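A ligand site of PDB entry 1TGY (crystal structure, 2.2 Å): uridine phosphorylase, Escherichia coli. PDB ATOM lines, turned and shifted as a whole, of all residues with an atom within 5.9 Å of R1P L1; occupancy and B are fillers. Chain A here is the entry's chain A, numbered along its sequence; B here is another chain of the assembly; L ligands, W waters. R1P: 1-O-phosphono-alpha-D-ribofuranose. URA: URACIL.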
ATOM      1  N   PRO A  28     -15.889  -8.669  -1.709  1.00  0.00           N
ATOM      2  CA  PRO A  28     -15.151  -8.943  -0.469  1.00  0.00           C
ATOM      3  C   PRO A  28     -13.978  -7.965  -0.401  1.00  0.00           C
ATOM      4  O   PRO A  28     -13.597  -7.376  -1.412  1.00  0.00           O
ATOM      5  CB  PRO A  28     -14.679 -10.377  -0.670  1.00  0.00           C
ATOM      6  CG  PRO A  28     -14.399 -10.414  -2.138  1.00  0.00           C
ATOM      7  CD  PRO A  28     -15.626  -9.718  -2.710  1.00  0.00           C
ATOM      8  N   GLY A  29     -13.414  -7.778   0.784  1.00  0.00           N
ATOM      9  CA  GLY A  29     -12.310  -6.854   0.906  1.00  0.00           C
ATOM     10  C   GLY A  29     -10.994  -7.474   0.501  1.00  0.00           C
ATOM     11  O   GLY A  29     -10.117  -6.804  -0.040  1.00  0.00           O
ATOM     12  N   ASP A  30     -10.864  -8.775   0.753  1.00  0.00           N
ATOM     13  CA  ASP A  30      -9.641  -9.515   0.448  1.00  0.00           C
ATOM     14  C   ASP A  30      -9.651 -10.227  -0.907  1.00  0.00           C
ATOM     15  O   ASP A  30     -10.550 -11.013  -1.200  1.00  0.00           O
ATOM     16  CB  ASP A  30      -9.399 -10.505   1.587  1.00  0.00           C
ATOM     17  CG  ASP A  30      -8.356 -11.540   1.259  1.00  0.00           C
ATOM     18  OD1 ASP A  30      -7.319 -11.169   0.675  1.00  0.00           O
ATOM     19  OD2 ASP A  30      -8.574 -12.718   1.595  1.00  0.00           O
ATOM     20  N   ARG A  33     -10.231 -13.968  -1.044  1.00  0.00           N
ATOM     21  CA  ARG A  33     -11.559 -14.516  -0.794  1.00  0.00           C
ATOM     22  C   ARG A  33     -12.420 -14.600  -2.064  1.00  0.00           C
ATOM     23  O   ARG A  33     -13.429 -15.315  -2.073  1.00  0.00           O
ATOM     24  CB  ARG A  33     -12.270 -13.684   0.272  1.00  0.00           C
ATOM     25  CG  ARG A  33     -13.558 -14.301   0.840  1.00  0.00           C
ATOM     26  CD  ARG A  33     -14.197 -13.348   1.843  1.00  0.00           C
ATOM     27  NE  ARG A  33     -13.234 -12.910   2.836  1.00  0.00           N
ATOM     28  CZ  ARG A  33     -13.170 -11.677   3.338  1.00  0.00           C
ATOM     29  NH1 ARG A  33     -14.020 -10.737   2.946  1.00  0.00           N
ATOM     30  NH2 ARG A  33     -12.223 -11.385   4.221  1.00  0.00           N
ATOM     31  N   GLY A  71     -10.290  -4.507  -1.764  1.00  0.00           N
ATOM     32  CA  GLY A  71      -9.072  -4.173  -1.076  1.00  0.00           C
ATOM     33  C   GLY A  71      -9.538  -3.524   0.213  1.00  0.00           C
ATOM     34  O   GLY A  71     -10.750  -3.375   0.432  1.00  0.00           O
ATOM     35  N   ILE A  72      -8.601  -3.125   1.075  1.00  0.00           N
ATOM     36  CA  ILE A  72      -8.975  -2.501   2.338  1.00  0.00           C
ATOM     37  C   ILE A  72      -9.194  -0.993   2.228  1.00  0.00           C
ATOM     38  O   ILE A  72      -8.338  -0.280   1.711  1.00  0.00           O
ATOM     39  CB  ILE A  72      -7.886  -2.729   3.417  1.00  0.00           C
ATOM     40  CG1 ILE A  72      -7.752  -4.219   3.737  1.00  0.00           C
ATOM     41  CG2 ILE A  72      -8.242  -1.959   4.678  1.00  0.00           C
ATOM     42  CD1 ILE A  72      -6.653  -4.539   4.743  1.00  0.00           C
ATOM     43  N   GLY A  73     -10.335  -0.513   2.706  1.00  0.00           N
ATOM     44  CA  GLY A  73     -10.595   0.911   2.685  1.00  0.00           C
ATOM     45  C   GLY A  73     -11.531   1.471   1.629  1.00  0.00           C
ATOM     46  O   GLY A  73     -11.657   0.950   0.507  1.00  0.00           O
ATOM     47  N   ARG A  94     -21.458  -6.663   0.034  1.00  0.00           N
ATOM     48  CA  ARG A  94     -20.138  -6.826   0.637  1.00  0.00           C
ATOM     49  C   ARG A  94     -20.154  -7.910   1.689  1.00  0.00           C
ATOM     50  O   ARG A  94     -21.086  -7.991   2.505  1.00  0.00           O
ATOM     51  CB  ARG A  94     -19.655  -5.516   1.283  1.00  0.00           C
ATOM     52  CG  ARG A  94     -18.391  -5.704   2.127  1.00  0.00           C
ATOM     53  CD  ARG A  94     -17.828  -4.382   2.655  1.00  0.00           C
ATOM     54  NE  ARG A  94     -17.223  -4.535   3.981  1.00  0.00           N
ATOM     55  CZ  ARG A  94     -16.156  -5.275   4.257  1.00  0.00           C
ATOM     56  NH1 ARG A  94     -15.532  -5.935   3.287  1.00  0.00           N
ATOM     57  NH2 ARG A  94     -15.722  -5.386   5.505  1.00  0.00           N
ATOM     58  N   ILE A  95     -19.136  -8.764   1.665  1.00  0.00           N
ATOM     59  CA  ILE A  95     -19.002  -9.824   2.650  1.00  0.00           C
ATOM     60  C   ILE A  95     -17.585  -9.660   3.190  1.00  0.00           C
ATOM     61  O   ILE A  95     -16.606  -9.753   2.447  1.00  0.00           O
ATOM     62  CB  ILE A  95     -19.220 -11.239   2.019  1.00  0.00           C
ATOM     63  CG1 ILE A  95     -19.161 -12.326   3.104  1.00  0.00           C
ATOM     64  CG2 ILE A  95     -18.186 -11.505   0.922  1.00  0.00           C
ATOM     65  CD1 ILE A  95     -17.764 -12.640   3.613  1.00  0.00           C
ATOM     66  N   GLY A  96     -17.468  -9.373   4.489  1.00  0.00           N
ATOM     67  CA  GLY A  96     -16.154  -9.189   5.066  1.00  0.00           C
ATOM     68  C   GLY A  96     -15.957  -9.807   6.434  1.00  0.00           C
ATOM     69  O   GLY A  96     -16.697 -10.703   6.844  1.00  0.00           O
ATOM     70  N   THR A  97     -14.921  -9.335   7.108  1.00  0.00           N
ATOM     71  CA  THR A  97     -14.597  -9.780   8.453  1.00  0.00           C
ATOM     72  C   THR A  97     -14.797  -8.557   9.350  1.00  0.00           C
ATOM     73  O   THR A  97     -14.769  -7.419   8.875  1.00  0.00           O
ATOM     74  CB  THR A  97     -13.139 -10.277   8.559  1.00  0.00           C
ATOM     75  OG1 THR A  97     -12.248  -9.284   8.033  1.00  0.00           O
ATOM     76  CG2 THR A  97     -12.983 -11.586   7.773  1.00  0.00           C
ATOM     77  N   THR A  98     -15.003  -8.790  10.644  1.00  0.00           N
ATOM     78  CA  THR A  98     -15.230  -7.663  11.532  1.00  0.00           C
ATOM     79  C   THR A  98     -14.915  -7.954  12.986  1.00  0.00           C
ATOM     80  O   THR A  98     -14.842  -9.121  13.410  1.00  0.00           O
ATOM     81  CB  THR A  98     -16.706  -7.214  11.412  1.00  0.00           C
ATOM     82  OG1 THR A  98     -16.922  -6.044  12.214  1.00  0.00           O
ATOM     83  CG2 THR A  98     -17.644  -8.334  11.889  1.00  0.00           C
ATOM     84  N   PHE A 165      -7.454   0.814  10.838  1.00  0.00           N
ATOM     85  CA  PHE A 165      -7.584  -0.445  11.562  1.00  0.00           C
ATOM     86  C   PHE A 165      -7.186  -0.230  13.018  1.00  0.00           C
ATOM     87  O   PHE A 165      -7.726  -0.876  13.917  1.00  0.00           O
ATOM     88  CB  PHE A 165      -6.684  -1.512  10.950  1.00  0.00           C
ATOM     89  CG  PHE A 165      -6.819  -2.865  11.604  1.00  0.00           C
ATOM     90  CD1 PHE A 165      -7.833  -3.735  11.210  1.00  0.00           C
ATOM     91  CD2 PHE A 165      -5.966  -3.250  12.620  1.00  0.00           C
ATOM     92  CE1 PHE A 165      -7.983  -4.986  11.820  1.00  0.00           C
ATOM     93  CE2 PHE A 165      -6.097  -4.493  13.251  1.00  0.00           C
ATOM     94  CZ  PHE A 165      -7.107  -5.366  12.844  1.00  0.00           C
ATOM     95  N   GLN A 169     -10.161   2.592  15.459  1.00  0.00           N
ATOM     96  CA  GLN A 169     -10.847   1.511  16.158  1.00  0.00           C
ATOM     97  C   GLN A 169     -10.307   1.482  17.587  1.00  0.00           C
ATOM     98  O   GLN A 169     -10.401   0.477  18.291  1.00  0.00           O
ATOM     99  CB  GLN A 169     -10.598   0.178  15.437  1.00  0.00           C
ATOM    100  CG  GLN A 169     -11.238   0.103  14.051  1.00  0.00           C
ATOM    101  CD  GLN A 169     -11.148  -1.276  13.413  1.00  0.00           C
ATOM    102  OE1 GLN A 169     -11.303  -2.303  14.092  1.00  0.00           O
ATOM    103  NE2 GLN A 169     -10.895  -1.313  12.109  1.00  0.00           N
ATOM    104  N   TYR A 198     -16.822  -2.955  14.213  1.00  0.00           N
ATOM    105  CA  TYR A 198     -15.899  -2.093  13.469  1.00  0.00           C
ATOM    106  C   TYR A 198     -15.514  -2.832  12.190  1.00  0.00           C
ATOM    107  O   TYR A 198     -15.242  -4.040  12.227  1.00  0.00           O
ATOM    108  CB  TYR A 198     -14.588  -1.867  14.243  1.00  0.00           C
ATOM    109  CG  TYR A 198     -14.578  -0.788  15.300  1.00  0.00           C
ATOM    110  CD1 TYR A 198     -14.183  -1.074  16.600  1.00  0.00           C
ATOM    111  CD2 TYR A 198     -14.869   0.547  14.974  1.00  0.00           C
ATOM    112  CE1 TYR A 198     -14.069  -0.075  17.562  1.00  0.00           C
ATOM    113  CE2 TYR A 198     -14.758   1.563  15.932  1.00  0.00           C
ATOM    114  CZ  TYR A 198     -14.352   1.241  17.226  1.00  0.00           C
ATOM    115  OH  TYR A 198     -14.210   2.231  18.176  1.00  0.00           O
ATOM    116  N   GLU A 199     -15.498  -2.116  11.067  1.00  0.00           N
ATOM    117  CA  GLU A 199     -15.085  -2.677   9.785  1.00  0.00           C
ATOM    118  C   GLU A 199     -14.501  -1.483   9.027  1.00  0.00           C
ATOM    119  O   GLU A 199     -14.450  -0.382   9.590  1.00  0.00           O
ATOM    120  CB  GLU A 199     -16.270  -3.304   9.047  1.00  0.00           C
ATOM    121  CG  GLU A 199     -17.140  -2.308   8.293  1.00  0.00           C
ATOM    122  CD  GLU A 199     -17.247  -2.662   6.842  1.00  0.00           C
ATOM    123  OE1 GLU A 199     -16.216  -2.661   6.155  1.00  0.00           O
ATOM    124  OE2 GLU A 199     -18.357  -2.964   6.381  1.00  0.00           O
ATOM    125  N   MET A 200     -14.086  -1.659   7.776  1.00  0.00           N
ATOM    126  CA  MET A 200     -13.474  -0.525   7.075  1.00  0.00           C
ATOM    127  C   MET A 200     -13.947  -0.167   5.670  1.00  0.00           C
ATOM    128  O   MET A 200     -13.257   0.598   4.977  1.00  0.00           O
ATOM    129  CB  MET A 200     -11.951  -0.725   7.059  1.00  0.00           C
ATOM    130  CG  MET A 200     -11.321  -0.936   8.433  1.00  0.00           C
ATOM    131  SD  MET A 200      -9.556  -1.334   8.378  1.00  0.00           S
ATOM    132  CE  MET A 200      -8.868   0.248   7.836  1.00  0.00           C
ATOM    133  N   GLU A 201     -15.093  -0.683   5.223  1.00  0.00           N
ATOM    134  CA  GLU A 201     -15.577  -0.350   3.879  1.00  0.00           C
ATOM    135  C   GLU A 201     -17.059  -0.007   3.774  1.00  0.00           C
ATOM    136  O   GLU A 201     -17.458   0.664   2.820  1.00  0.00           O
ATOM    137  CB  GLU A 201     -15.279  -1.486   2.888  1.00  0.00           C
ATOM    138  CG  GLU A 201     -13.801  -1.782   2.600  1.00  0.00           C
ATOM    139  CD  GLU A 201     -13.128  -2.574   3.716  1.00  0.00           C
ATOM    140  OE1 GLU A 201     -13.793  -3.454   4.300  1.00  0.00           O
ATOM    141  OE2 GLU A 201     -11.936  -2.332   3.995  1.00  0.00           O
ATOM    142  N   PHE B  10      -0.519  -8.161  12.107  1.00  0.00           N
ATOM    143  CA  PHE B  10      -1.809  -8.658  11.676  1.00  0.00           C
ATOM    144  C   PHE B  10      -2.079  -8.818  10.171  1.00  0.00           C
ATOM    145  O   PHE B  10      -2.756  -9.761   9.773  1.00  0.00           O
ATOM    146  CB  PHE B  10      -2.933  -7.806  12.276  1.00  0.00           C
ATOM    147  CG  PHE B  10      -4.277  -8.473  12.237  1.00  0.00           C
ATOM    148  CD1 PHE B  10      -4.710  -9.279  13.287  1.00  0.00           C
ATOM    149  CD2 PHE B  10      -5.103  -8.327  11.117  1.00  0.00           C
ATOM    150  CE1 PHE B  10      -5.943  -9.922  13.237  1.00  0.00           C
ATOM    151  CE2 PHE B  10      -6.345  -8.975  11.057  1.00  0.00           C
ATOM    152  CZ  PHE B  10      -6.762  -9.769  12.117  1.00  0.00           C
ATOM    153  N   HIS B  11      -1.547  -7.918   9.343  1.00  0.00           N
ATOM    154  CA  HIS B  11      -1.816  -8.009   7.910  1.00  0.00           C
ATOM    155  C   HIS B  11      -0.648  -8.338   6.973  1.00  0.00           C
ATOM    156  O   HIS B  11      -0.820  -9.099   6.023  1.00  0.00           O
ATOM    157  CB  HIS B  11      -2.453  -6.703   7.404  1.00  0.00           C
ATOM    158  CG  HIS B  11      -3.696  -6.302   8.124  1.00  0.00           C
ATOM    159  ND1 HIS B  11      -3.680  -5.628   9.329  1.00  0.00           N
ATOM    160  CD2 HIS B  11      -5.004  -6.461   7.801  1.00  0.00           C
ATOM    161  CE1 HIS B  11      -4.925  -5.391   9.705  1.00  0.00           C
ATOM    162  NE2 HIS B  11      -5.751  -5.883   8.796  1.00  0.00           N
ATOM    163  N   ARG B  51      -3.227  -9.980   0.725  1.00  0.00           N
ATOM    164  CA  ARG B  51      -4.136  -8.898   0.374  1.00  0.00           C
ATOM    165  C   ARG B  51      -3.375  -7.994  -0.597  1.00  0.00           C
ATOM    166  O   ARG B  51      -2.704  -8.492  -1.493  1.00  0.00           O
ATOM    167  CB  ARG B  51      -4.566  -8.130   1.633  1.00  0.00           C
ATOM    168  CG  ARG B  51      -5.570  -8.898   2.516  1.00  0.00           C
ATOM    169  CD  ARG B  51      -5.814  -8.169   3.829  1.00  0.00           C
ATOM    170  NE  ARG B  51      -6.854  -8.786   4.639  1.00  0.00           N
ATOM    171  CZ  ARG B  51      -8.160  -8.618   4.469  1.00  0.00           C
ATOM    172  NH1 ARG B  51      -8.614  -7.827   3.501  1.00  0.00           N
ATOM    173  NH2 ARG B  51      -9.030  -9.212   5.272  1.00  0.00           N
ATOM    174  N   ILE B  79      -2.346   0.935   7.519  1.00  0.00           N
ATOM    175  CA  ILE B  79      -2.074  -0.397   8.042  1.00  0.00           C
ATOM    176  C   ILE B  79      -0.623  -0.777   7.750  1.00  0.00           C
ATOM    177  O   ILE B  79       0.110  -1.198   8.641  1.00  0.00           O
ATOM    178  CB  ILE B  79      -3.015  -1.446   7.399  1.00  0.00           C
ATOM    179  CG1 ILE B  79      -4.414  -1.323   8.018  1.00  0.00           C
ATOM    180  CG2 ILE B  79      -2.457  -2.862   7.571  1.00  0.00           C
ATOM    181  CD1 ILE B  79      -5.441  -2.231   7.400  1.00  0.00           C
HETATM  182  C5  R1P L   1      -9.274  -5.301   8.203  1.00  0.00           C
HETATM  183  O5  R1P L   1      -8.471  -6.426   8.578  1.00  0.00           O
HETATM  184  C4  R1P L   1      -9.996  -5.626   6.896  1.00  0.00           C
HETATM  185  O4  R1P L   1     -10.870  -6.764   7.012  1.00  0.00           O
HETATM  186  C1  R1P L   1     -12.243  -6.315   7.086  1.00  0.00           C
HETATM  187  C2  R1P L   1     -12.152  -4.793   7.205  1.00  0.00           C
HETATM  188  O2  R1P L   1     -13.315  -4.138   6.699  1.00  0.00           O
HETATM  189  C3  R1P L   1     -10.889  -4.483   6.397  1.00  0.00           C
HETATM  190  O3  R1P L   1     -11.148  -4.643   5.001  1.00  0.00           O
HETATM  191  O1  R1P L   1     -12.943  -6.661   5.887  1.00  0.00           O
HETATM  192  P   R1P L   1     -12.314  -7.613   4.753  1.00  0.00           P
HETATM  193  O1P R1P L   1     -13.391  -8.024   3.815  1.00  0.00           O
HETATM  194  O2P R1P L   1     -11.098  -6.975   4.203  1.00  0.00           O
HETATM  195  O3P R1P L   1     -11.850  -8.918   5.577  1.00  0.00           O
HETATM  196  N1  URA L   2     -11.578  -6.003  10.592  1.00  0.00           N
HETATM  197  C2  URA L   2     -11.670  -4.726  11.201  1.00  0.00           C
HETATM  198  O2  URA L   2     -11.928  -3.681  10.614  1.00  0.00           O
HETATM  199  N3  URA L   2     -11.463  -4.732  12.567  1.00  0.00           N
HETATM  200  C4  URA L   2     -11.170  -5.832  13.401  1.00  0.00           C
HETATM  201  O4  URA L   2     -10.982  -5.815  14.637  1.00  0.00           O
HETATM  202  C5  URA L   2     -11.092  -7.106  12.674  1.00  0.00           C
HETATM  203  C6  URA L   2     -11.294  -7.148  11.332  1.00  0.00           C
HETATM  204  O   HOH W   1      -9.468  -8.887   9.167  1.00  0.00           O
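An oxygen (O2) of R1P L1 is in hydrogen-bond range of the side-chain carboxylate (OE1) of Glu 201 (2.5 Å).
The backbone NH of Gly 29 is in hydrogen-bond range of an oxygen (O1P) of R1P L1, at 3.0 Å.
The guanidinium group (NH2) of Arg 33 lies within salt-bridge range of an oxygen (O3P) of R1P L1 (2.8 Å).
The guanidinium group (NH1) of Arg 51 of chain B lies within salt-bridge range of an oxygen (O2P) of R1P L1.
O3P of R1P L1 is in hydrogen-bond range of OG1 of Thr 97.
The side-chain carboxylate (OE1) of Glu 199 is in hydrogen-bond range of an oxygen (O2) of R1P L1, 3.3 Å away.
An oxygen (O5) of R1P L1 is in hydrogen-bond range of a ring nitrogen (NE2) of His 11 of chain B, at 2.8 Å.
A nitrogen (N3) of URA L2 sits at hydrogen-bond distance from the side-chain amide oxygen (OE1) of Gln 169.
The backbone NH (N) of Met 200 is in hydrogen-bond range of an oxygen (O2) of R1P L1 (2.8 Å).
NH1 of Arg 94 lies within salt-bridge range of O1P of R1P L1, at 3.0 Å.
The backbone NH (N) of Thr 97 is in hydrogen-bond range of an oxygen (O3P) of R1P L1 (3.5 Å).
The guanidinium group (NH2) of Arg 94 is in salt-bridge range of the side-chain carboxylate (OE1) of Glu 201, 3.0 Å away.
The backbone NH (N) of Glu 201 sits at hydrogen-bond distance from the side-chain carboxylate (OE1) of Glu 199 (2.5 Å).
The side-chain carboxylate of Glu 201 lies within hydrogen-bond range of the backbone NH of Gly 73, 2.7 Å away.
The backbone NH of Gly 71 is in hydrogen-bond range of the backbone carbonyl oxygen of Gly 29 (2.9 Å).
The guanidinium group (NH1) of Arg 33 lies within hydrogen-bond range of the backbone carbonyl oxygen (O) of Ile 95, at 2.8 Å.
The guanidinium group (NH2) of Arg 94 lies within salt-bridge range of the side-chain carboxylate (OE1) of Glu 199.
The backbone NH (N) of Arg 33 lies within hydrogen-bond range of the side-chain carboxylate (OD2) of Asp 30.
Residues that only touch R1P L1: Asp 30, Ile 72, Ile 95, Gly 96 and Phe 165.
Hydrophobic or aromatic side chains within 4 Å of R1P L1: Ile 72, Phe 165, Met 200 and His 11 of chain B.
14 residues have an atom within 4 Å of R1P L1: Gly 29, Asp 30, Arg 33, Ile 72, Arg 94, Ile 95, Gly 96, Thr 97, Phe 165, Glu 199, Met 200, Glu 201, His 11 of chain B and Arg 51 of chain B.
The nearest printed residue that does not touch R1P L1 is Phe 10 of chain B (4.1 Å).
Water W1 lies within hydrogen-bond range of O5 of R1P L1 (2.7 Å) and OG1 of Thr 97 (3.0 Å).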
